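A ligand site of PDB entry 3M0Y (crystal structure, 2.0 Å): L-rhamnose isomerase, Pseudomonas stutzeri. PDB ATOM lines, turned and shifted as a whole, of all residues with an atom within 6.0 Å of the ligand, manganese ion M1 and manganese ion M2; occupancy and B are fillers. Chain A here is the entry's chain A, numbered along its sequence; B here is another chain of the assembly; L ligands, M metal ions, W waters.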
ATOM      1  N   TRP A  57     -32.112 -18.212  27.791  1.00  0.00           N
ATOM      2  CA  TRP A  57     -32.475 -19.537  28.276  1.00  0.00           C
ATOM      3  C   TRP A  57     -31.730 -20.019  29.526  1.00  0.00           C
ATOM      4  O   TRP A  57     -32.006 -21.099  30.048  1.00  0.00           O
ATOM      5  CB  TRP A  57     -32.326 -20.559  27.145  1.00  0.00           C
ATOM      6  CG  TRP A  57     -30.917 -20.722  26.615  1.00  0.00           C
ATOM      7  CD1 TRP A  57     -29.953 -21.576  27.070  1.00  0.00           C
ATOM      8  CD2 TRP A  57     -30.324 -20.008  25.518  1.00  0.00           C
ATOM      9  NE1 TRP A  57     -28.802 -21.435  26.339  1.00  0.00           N
ATOM     10  CE2 TRP A  57     -28.995 -20.486  25.379  1.00  0.00           C
ATOM     11  CE3 TRP A  57     -30.774 -19.006  24.649  1.00  0.00           C
ATOM     12  CZ2 TRP A  57     -28.124 -19.993  24.402  1.00  0.00           C
ATOM     13  CZ3 TRP A  57     -29.911 -18.517  23.676  1.00  0.00           C
ATOM     14  CH2 TRP A  57     -28.595 -19.023  23.559  1.00  0.00           C
ATOM     15  N   HIS A 101     -33.667 -16.974  21.877  1.00  0.00           N
ATOM     16  CA  HIS A 101     -33.946 -18.282  21.308  1.00  0.00           C
ATOM     17  C   HIS A 101     -35.389 -18.325  20.820  1.00  0.00           C
ATOM     18  O   HIS A 101     -36.309 -18.010  21.569  1.00  0.00           O
ATOM     19  CB  HIS A 101     -33.721 -19.367  22.375  1.00  0.00           C
ATOM     20  CG  HIS A 101     -33.054 -20.605  21.848  1.00  0.00           C
ATOM     21  ND1 HIS A 101     -33.604 -21.382  20.844  1.00  0.00           N
ATOM     22  CD2 HIS A 101     -31.860 -21.174  22.150  1.00  0.00           C
ATOM     23  CE1 HIS A 101     -32.779 -22.372  20.563  1.00  0.00           C
ATOM     24  NE2 HIS A 101     -31.717 -22.278  21.343  1.00  0.00           N
ATOM     25  N   TRP A 104     -38.908 -19.997  21.818  1.00  0.00           N
ATOM     26  CA  TRP A 104     -39.004 -19.736  23.247  1.00  0.00           C
ATOM     27  C   TRP A 104     -39.262 -18.270  23.599  1.00  0.00           C
ATOM     28  O   TRP A 104     -40.149 -17.957  24.400  1.00  0.00           O
ATOM     29  CB  TRP A 104     -37.729 -20.178  23.983  1.00  0.00           C
ATOM     30  CG  TRP A 104     -37.489 -21.661  23.981  1.00  0.00           C
ATOM     31  CD1 TRP A 104     -38.421 -22.644  23.787  1.00  0.00           C
ATOM     32  CD2 TRP A 104     -36.243 -22.324  24.226  1.00  0.00           C
ATOM     33  NE1 TRP A 104     -37.827 -23.874  23.898  1.00  0.00           N
ATOM     34  CE2 TRP A 104     -36.492 -23.710  24.163  1.00  0.00           C
ATOM     35  CE3 TRP A 104     -34.942 -21.878  24.488  1.00  0.00           C
ATOM     36  CZ2 TRP A 104     -35.490 -24.669  24.362  1.00  0.00           C
ATOM     37  CZ3 TRP A 104     -33.934 -22.823  24.689  1.00  0.00           C
ATOM     38  CH2 TRP A 104     -34.220 -24.210  24.623  1.00  0.00           C
ATOM     39  N   ASN A 127     -30.908 -17.393  17.885  1.00  0.00           N
ATOM     40  CA  ASN A 127     -30.715 -18.830  17.948  1.00  0.00           C
ATOM     41  C   ASN A 127     -31.982 -19.520  17.473  1.00  0.00           C
ATOM     42  O   ASN A 127     -33.054 -19.281  18.013  1.00  0.00           O
ATOM     43  CB  ASN A 127     -30.409 -19.278  19.388  1.00  0.00           C
ATOM     44  CG  ASN A 127     -29.075 -18.785  19.884  1.00  0.00           C
ATOM     45  OD1 ASN A 127     -28.052 -19.460  19.740  1.00  0.00           O
ATOM     46  ND2 ASN A 127     -29.064 -17.607  20.483  1.00  0.00           N
ATOM     47  N   SER A 128     -31.847 -20.378  16.472  1.00  0.00           N
ATOM     48  CA  SER A 128     -32.998 -21.112  15.953  1.00  0.00           C
ATOM     49  C   SER A 128     -33.192 -22.398  16.758  1.00  0.00           C
ATOM     50  O   SER A 128     -32.253 -22.894  17.395  1.00  0.00           O
ATOM     51  CB  SER A 128     -32.805 -21.448  14.482  1.00  0.00           C
ATOM     52  OG  SER A 128     -31.630 -22.213  14.296  1.00  0.00           O
ATOM     53  N   PHE A 131     -34.729 -28.516  17.142  1.00  0.00           N
ATOM     54  CA  PHE A 131     -34.349 -29.703  17.888  1.00  0.00           C
ATOM     55  C   PHE A 131     -35.491 -30.115  18.842  1.00  0.00           C
ATOM     56  O   PHE A 131     -35.343 -31.006  19.678  1.00  0.00           O
ATOM     57  CB  PHE A 131     -33.039 -29.479  18.649  1.00  0.00           C
ATOM     58  CG  PHE A 131     -33.058 -28.305  19.586  1.00  0.00           C
ATOM     59  CD1 PHE A 131     -33.761 -28.362  20.789  1.00  0.00           C
ATOM     60  CD2 PHE A 131     -32.390 -27.116  19.255  1.00  0.00           C
ATOM     61  CE1 PHE A 131     -33.800 -27.273  21.652  1.00  0.00           C
ATOM     62  CE2 PHE A 131     -32.421 -26.023  20.114  1.00  0.00           C
ATOM     63  CZ  PHE A 131     -33.118 -26.097  21.309  1.00  0.00           C
ATOM     64  N   THR A 177     -27.333 -18.158  14.966  1.00  0.00           N
ATOM     65  CA  THR A 177     -26.582 -19.336  15.385  1.00  0.00           C
ATOM     66  C   THR A 177     -27.453 -20.555  15.143  1.00  0.00           C
ATOM     67  O   THR A 177     -28.615 -20.593  15.567  1.00  0.00           O
ATOM     68  CB  THR A 177     -26.216 -19.282  16.870  1.00  0.00           C
ATOM     69  OG1 THR A 177     -25.271 -18.221  17.081  1.00  0.00           O
ATOM     70  CG2 THR A 177     -25.597 -20.608  17.331  1.00  0.00           C
ATOM     71  N   TRP A 179     -27.710 -24.551  15.785  1.00  0.00           N
ATOM     72  CA  TRP A 179     -27.309 -25.792  16.419  1.00  0.00           C
ATOM     73  C   TRP A 179     -28.504 -26.704  16.300  1.00  0.00           C
ATOM     74  O   TRP A 179     -29.619 -26.304  16.651  1.00  0.00           O
ATOM     75  CB  TRP A 179     -26.983 -25.623  17.902  1.00  0.00           C
ATOM     76  CG  TRP A 179     -26.746 -26.958  18.542  1.00  0.00           C
ATOM     77  CD1 TRP A 179     -25.643 -27.758  18.398  1.00  0.00           C
ATOM     78  CD2 TRP A 179     -27.683 -27.710  19.335  1.00  0.00           C
ATOM     79  NE1 TRP A 179     -25.839 -28.962  19.039  1.00  0.00           N
ATOM     80  CE2 TRP A 179     -27.079 -28.956  19.627  1.00  0.00           C
ATOM     81  CE3 TRP A 179     -28.968 -27.449  19.825  1.00  0.00           C
ATOM     82  CZ2 TRP A 179     -27.727 -29.938  20.377  1.00  0.00           C
ATOM     83  CZ3 TRP A 179     -29.603 -28.429  20.580  1.00  0.00           C
ATOM     84  CH2 TRP A 179     -28.980 -29.659  20.853  1.00  0.00           C
ATOM     85  N   GLU A 219     -22.862 -24.499  14.874  1.00  0.00           N
ATOM     86  CA  GLU A 219     -22.290 -25.039  16.098  1.00  0.00           C
ATOM     87  C   GLU A 219     -22.152 -26.557  16.096  1.00  0.00           C
ATOM     88  O   GLU A 219     -23.140 -27.282  16.024  1.00  0.00           O
ATOM     89  CB  GLU A 219     -23.153 -24.594  17.283  1.00  0.00           C
ATOM     90  CG  GLU A 219     -22.753 -25.172  18.629  1.00  0.00           C
ATOM     91  CD  GLU A 219     -23.520 -24.557  19.774  1.00  0.00           C
ATOM     92  OE1 GLU A 219     -24.562 -23.915  19.526  1.00  0.00           O
ATOM     93  OE2 GLU A 219     -23.095 -24.719  20.935  1.00  0.00           O
ATOM     94  N   LYS A 221     -21.174 -30.335  17.695  1.00  0.00           N
ATOM     95  CA  LYS A 221     -21.334 -31.024  18.970  1.00  0.00           C
ATOM     96  C   LYS A 221     -21.106 -32.518  18.746  1.00  0.00           C
ATOM     97  O   LYS A 221     -21.727 -33.130  17.880  1.00  0.00           O
ATOM     98  CB  LYS A 221     -22.733 -30.784  19.540  1.00  0.00           C
ATOM     99  CG  LYS A 221     -22.875 -31.241  20.994  1.00  0.00           C
ATOM    100  CD  LYS A 221     -24.271 -30.969  21.526  1.00  0.00           C
ATOM    101  CE  LYS A 221     -24.395 -31.334  22.997  1.00  0.00           C
ATOM    102  NZ  LYS A 221     -25.795 -31.166  23.499  1.00  0.00           N
ATOM    103  N   GLU A 224     -25.299 -35.956  21.795  1.00  0.00           N
ATOM    104  CA  GLU A 224     -26.438 -35.454  22.583  1.00  0.00           C
ATOM    105  C   GLU A 224     -27.114 -34.335  21.794  1.00  0.00           C
ATOM    106  O   GLU A 224     -26.529 -33.274  21.591  1.00  0.00           O
ATOM    107  CB  GLU A 224     -26.021 -34.909  23.961  1.00  0.00           C
ATOM    108  CG  GLU A 224     -27.248 -34.450  24.773  1.00  0.00           C
ATOM    109  CD  GLU A 224     -26.925 -33.676  26.048  1.00  0.00           C
ATOM    110  OE1 GLU A 224     -26.029 -32.808  26.027  1.00  0.00           O
ATOM    111  OE2 GLU A 224     -27.597 -33.924  27.070  1.00  0.00           O
ATOM    112  N   LEU A 252     -18.936 -21.794  15.347  1.00  0.00           N
ATOM    113  CA  LEU A 252     -19.087 -21.400  16.730  1.00  0.00           C
ATOM    114  C   LEU A 252     -18.552 -22.550  17.577  1.00  0.00           C
ATOM    115  O   LEU A 252     -18.920 -23.710  17.377  1.00  0.00           O
ATOM    116  CB  LEU A 252     -20.554 -21.115  17.044  1.00  0.00           C
ATOM    117  CG  LEU A 252     -20.813 -20.556  18.443  1.00  0.00           C
ATOM    118  CD1 LEU A 252     -21.919 -19.517  18.362  1.00  0.00           C
ATOM    119  CD2 LEU A 252     -21.164 -21.688  19.395  1.00  0.00           C
ATOM    120  N   ASP A 254     -18.394 -24.265  21.157  1.00  0.00           N
ATOM    121  CA  ASP A 254     -18.969 -24.375  22.485  1.00  0.00           C
ATOM    122  C   ASP A 254     -17.995 -25.306  23.220  1.00  0.00           C
ATOM    123  O   ASP A 254     -17.840 -26.477  22.862  1.00  0.00           O
ATOM    124  CB  ASP A 254     -20.381 -24.974  22.430  1.00  0.00           C
ATOM    125  CG  ASP A 254     -21.036 -25.047  23.792  1.00  0.00           C
ATOM    126  OD1 ASP A 254     -22.227 -24.692  23.923  1.00  0.00           O
ATOM    127  OD2 ASP A 254     -20.354 -25.476  24.749  1.00  0.00           O
ATOM    128  N   HIS A 257     -18.527 -29.166  23.964  1.00  0.00           N
ATOM    129  CA  HIS A 257     -18.967 -30.035  22.869  1.00  0.00           C
ATOM    130  C   HIS A 257     -17.874 -30.873  22.232  1.00  0.00           C
ATOM    131  O   HIS A 257     -18.030 -31.303  21.085  1.00  0.00           O
ATOM    132  CB  HIS A 257     -19.616 -29.196  21.767  1.00  0.00           C
ATOM    133  CG  HIS A 257     -20.934 -28.601  22.150  1.00  0.00           C
ATOM    134  ND1 HIS A 257     -21.781 -28.022  21.224  1.00  0.00           N
ATOM    135  CD2 HIS A 257     -21.553 -28.485  23.346  1.00  0.00           C
ATOM    136  CE1 HIS A 257     -22.866 -27.592  21.841  1.00  0.00           C
ATOM    137  NE2 HIS A 257     -22.755 -27.864  23.123  1.00  0.00           N
ATOM    138  N   HIS A 281     -19.202 -20.219  22.849  1.00  0.00           N
ATOM    139  CA  HIS A 281     -20.297 -20.488  23.784  1.00  0.00           C
ATOM    140  C   HIS A 281     -19.477 -20.914  24.997  1.00  0.00           C
ATOM    141  O   HIS A 281     -18.898 -21.995  25.031  1.00  0.00           O
ATOM    142  CB  HIS A 281     -21.207 -21.621  23.294  1.00  0.00           C
ATOM    143  CG  HIS A 281     -22.418 -21.144  22.556  1.00  0.00           C
ATOM    144  ND1 HIS A 281     -23.463 -21.980  22.221  1.00  0.00           N
ATOM    145  CD2 HIS A 281     -22.764 -19.915  22.101  1.00  0.00           C
ATOM    146  CE1 HIS A 281     -24.397 -21.287  21.593  1.00  0.00           C
ATOM    147  NE2 HIS A 281     -23.991 -20.038  21.501  1.00  0.00           N
ATOM    148  N   ASN A 283     -18.666 -21.976  28.889  1.00  0.00           N
ATOM    149  CA  ASN A 283     -19.194 -22.793  29.978  1.00  0.00           C
ATOM    150  C   ASN A 283     -18.052 -23.702  30.410  1.00  0.00           C
ATOM    151  O   ASN A 283     -16.954 -23.622  29.857  1.00  0.00           O
ATOM    152  CB  ASN A 283     -20.406 -23.611  29.493  1.00  0.00           C
ATOM    153  CG  ASN A 283     -20.128 -24.395  28.230  1.00  0.00           C
ATOM    154  OD1 ASN A 283     -19.232 -25.231  28.181  1.00  0.00           O
ATOM    155  ND2 ASN A 283     -20.914 -24.124  27.189  1.00  0.00           N
ATOM    156  N   ASP A 289     -21.248 -32.492  27.874  1.00  0.00           N
ATOM    157  CA  ASP A 289     -21.655 -31.104  27.692  1.00  0.00           C
ATOM    158  C   ASP A 289     -22.394 -30.708  28.970  1.00  0.00           C
ATOM    159  O   ASP A 289     -23.615 -30.485  28.970  1.00  0.00           O
ATOM    160  CB  ASP A 289     -22.549 -30.982  26.453  1.00  0.00           C
ATOM    161  CG  ASP A 289     -23.013 -29.558  26.208  1.00  0.00           C
ATOM    162  OD1 ASP A 289     -22.253 -28.613  26.524  1.00  0.00           O
ATOM    163  OD2 ASP A 289     -24.129 -29.388  25.681  1.00  0.00           O
ATOM    164  N   ASP A 291     -22.386 -27.970  30.707  1.00  0.00           N
ATOM    165  CA  ASP A 291     -22.906 -26.614  30.770  1.00  0.00           C
ATOM    166  C   ASP A 291     -22.796 -25.936  32.137  1.00  0.00           C
ATOM    167  O   ASP A 291     -23.712 -25.224  32.564  1.00  0.00           O
ATOM    168  CB  ASP A 291     -24.382 -26.609  30.327  1.00  0.00           C
ATOM    169  CG  ASP A 291     -24.546 -26.735  28.824  1.00  0.00           C
ATOM    170  OD1 ASP A 291     -23.837 -25.995  28.108  1.00  0.00           O
ATOM    171  OD2 ASP A 291     -25.377 -27.550  28.360  1.00  0.00           O
ATOM    172  N   ASP A 327     -23.238 -19.977  27.301  1.00  0.00           N
ATOM    173  CA  ASP A 327     -24.290 -20.954  27.057  1.00  0.00           C
ATOM    174  C   ASP A 327     -24.162 -21.929  28.213  1.00  0.00           C
ATOM    175  O   ASP A 327     -23.379 -22.872  28.160  1.00  0.00           O
ATOM    176  CB  ASP A 327     -24.093 -21.700  25.733  1.00  0.00           C
ATOM    177  CG  ASP A 327     -25.190 -22.742  25.471  1.00  0.00           C
ATOM    178  OD1 ASP A 327     -26.133 -22.836  26.301  1.00  0.00           O
ATOM    179  OD2 ASP A 327     -25.107 -23.454  24.448  1.00  0.00           O
ATOM    180  N   ARG B  65     -32.741 -34.017  27.553  1.00  0.00           N
ATOM    181  CA  ARG B  65     -33.046 -32.726  28.152  1.00  0.00           C
ATOM    182  C   ARG B  65     -33.519 -31.725  27.106  1.00  0.00           C
ATOM    183  O   ARG B  65     -34.130 -30.710  27.439  1.00  0.00           O
ATOM    184  CB  ARG B  65     -31.826 -32.164  28.877  1.00  0.00           C
ATOM    185  CG  ARG B  65     -30.602 -31.968  28.014  1.00  0.00           C
ATOM    186  CD  ARG B  65     -29.460 -31.358  28.821  1.00  0.00           C
ATOM    187  NE  ARG B  65     -28.219 -31.321  28.055  1.00  0.00           N
ATOM    188  CZ  ARG B  65     -27.299 -30.364  28.153  1.00  0.00           C
ATOM    189  NH1 ARG B  65     -27.492 -29.348  28.985  1.00  0.00           N
ATOM    190  NH2 ARG B  65     -26.207 -30.413  27.410  1.00  0.00           N
ATOM    191  N   PHE B  66     -33.246 -31.993  25.835  1.00  0.00           N
ATOM    192  CA  PHE B  66     -33.648 -31.096  24.765  1.00  0.00           C
ATOM    193  C   PHE B  66     -35.055 -31.343  24.242  1.00  0.00           C
ATOM    194  O   PHE B  66     -35.749 -30.404  23.849  1.00  0.00           O
ATOM    195  CB  PHE B  66     -32.647 -31.172  23.613  1.00  0.00           C
ATOM    196  CG  PHE B  66     -31.300 -30.636  23.960  1.00  0.00           C
ATOM    197  CD1 PHE B  66     -31.089 -29.260  24.065  1.00  0.00           C
ATOM    198  CD2 PHE B  66     -30.243 -31.498  24.216  1.00  0.00           C
ATOM    199  CE1 PHE B  66     -29.850 -28.757  24.428  1.00  0.00           C
ATOM    200  CE2 PHE B  66     -28.988 -31.002  24.580  1.00  0.00           C
ATOM    201  CZ  PHE B  66     -28.801 -29.624  24.688  1.00  0.00           C
HETATM  202  C1  LIG L   1     -26.669 -27.534  22.618  1.00  0.00           C
HETATM  203  C2  LIG L   1     -25.948 -26.255  22.237  1.00  0.00           C
HETATM  204  C3  LIG L   1     -26.947 -25.157  21.876  1.00  0.00           C
HETATM  205  C4  LIG L   1     -28.082 -25.086  22.900  1.00  0.00           C
HETATM  206  C5  LIG L   1     -28.884 -23.806  22.732  1.00  0.00           C
HETATM  207  C6  LIG L   1     -29.999 -23.761  23.772  1.00  0.00           C
HETATM  208  O1  LIG L   1     -26.045 -28.460  23.149  1.00  0.00           O
HETATM  209  O2  LIG L   1     -25.142 -25.818  23.326  1.00  0.00           O
HETATM  210  O3  LIG L   1     -26.288 -23.913  21.805  1.00  0.00           O
HETATM  211  O4  LIG L   1     -27.544 -25.138  24.220  1.00  0.00           O
HETATM  212  O5  LIG L   1     -29.450 -23.760  21.426  1.00  0.00           O
HETATM  213 MN    MN M   1     -23.968 -24.018  22.797  1.00  0.00          MN
HETATM  214 MN    MN M   2     -24.500 -27.689  24.454  1.00  0.00          MN
HETATM  215  O   HOH W   1     -23.441 -26.480  25.833  1.00  0.00           O
HETATM  216  O   HOH W   2     -28.113 -22.424  19.570  1.00  0.00           O
HETATM  217  O   HOH W   3     -26.128 -27.294  25.892  1.00  0.00           O
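NE2 of His 101 lies within hydrogen-bond range of O5 of the ligand (2.7 Å). An oxygen (O1) of the ligand sits close to the side-chain amino group (NZ) of Lys 221 (2.7 Å).
OD1 of Asp 327 lies within hydrogen-bond range of NE1 of Trp 57 (3.0 Å). ND2 of Asn 283 lies within hydrogen-bond range of O of Asp 327 (2.9 Å). The side-chain carboxylate (OD2) of Asp 289 sits close to the side-chain amino group (NZ) of Lys 221 (3.3 Å). NH2 of Arg 65 of chain B sits at hydrogen-bond distance from O of Asp 289 (3.0 Å). The side-chain amide nitrogen of Asn 283 is in hydrogen-bond range of the side-chain carboxylate of Asp 254 (2.8 Å). OE1 of Glu 224 lies within salt-bridge range of NZ of Lys 221.
Merely in contact with the ligand: Trp 179 (3.3 Å), Phe 66 of chain B (3.4 Å), Trp 57 (3.7 Å) and Phe 131 (3.96 Å). Hydrophobic or aromatic side chains that line the ligand: Trp 57, His 101, Phe 131, Trp 179, His 257, His 281 and Phe 66 of chain B. Of the 21 residues printed, 12 come within 4 Å of the ligand. Along chain A the residues within 4 Å of the ligand span positions 57 to 327. The nearest printed residue that does not touch the ligand is Trp 104 (4.1 Å).
Within 4 Å of manganese ion M1: Glu 219, Asp 254, His 257, His 281 and Asp 327. Along chain A the residues within 4 Å of manganese ion M1 span positions 219 to 327. The nearest printed residue that does not touch manganese ion M1 is Leu 252 (5.0 Å).
Lys 221 touches manganese ion M2 (NZ to MN, 3.8 Å). Four residues have an atom within 4 Å of manganese ion M2: Lys 221, Asp 254, His 257 and Asp 289. Along chain A the residues within 4 Å of manganese ion M2 span positions 221 to 289. The nearest printed residue that does not touch manganese ion M2 is Asp 291 (4.01 Å).
Manganese ion M1 is bound by the side-chain carboxylate of Asp 327 (2.1 Å), the side-chain carboxylate of Glu 219 (2.2 Å), a ring nitrogen (ND1) of His 281 (2.2 Å), the side-chain carboxylate of Asp 254 (2.2 Å), an oxygen (O2) of the ligand (2.2 Å) and an oxygen (O3) of the ligand (2.5 Å).
Manganese ion M2 is bound by water W1, 2.1 Å away. OD2 of Asp 289 binds manganese ion M2 (2.1 Å). An oxygen (O1) of the ligand binds manganese ion M2. Manganese ion M2 is bound by NE2 of His 257 (2.2 Å). Water W3 binds manganese ion M2 (2.2 Å). O2 of the ligand is bound to manganese ion M2 (2.3 Å). Manganese ion M2 has six donor atoms within binding distance.
Water W3 lies within hydrogen-bond range of OD2 of Asp 291 (2.6 Å), O4 of the ligand (3.1 Å) and NH2 of Arg 65 of chain B (3.5 Å). Water W2 bridges an oxygen (O5) of the ligand (2.6 Å) and the side-chain amide oxygen (OD1) of Asn 127 (3.0 Å).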
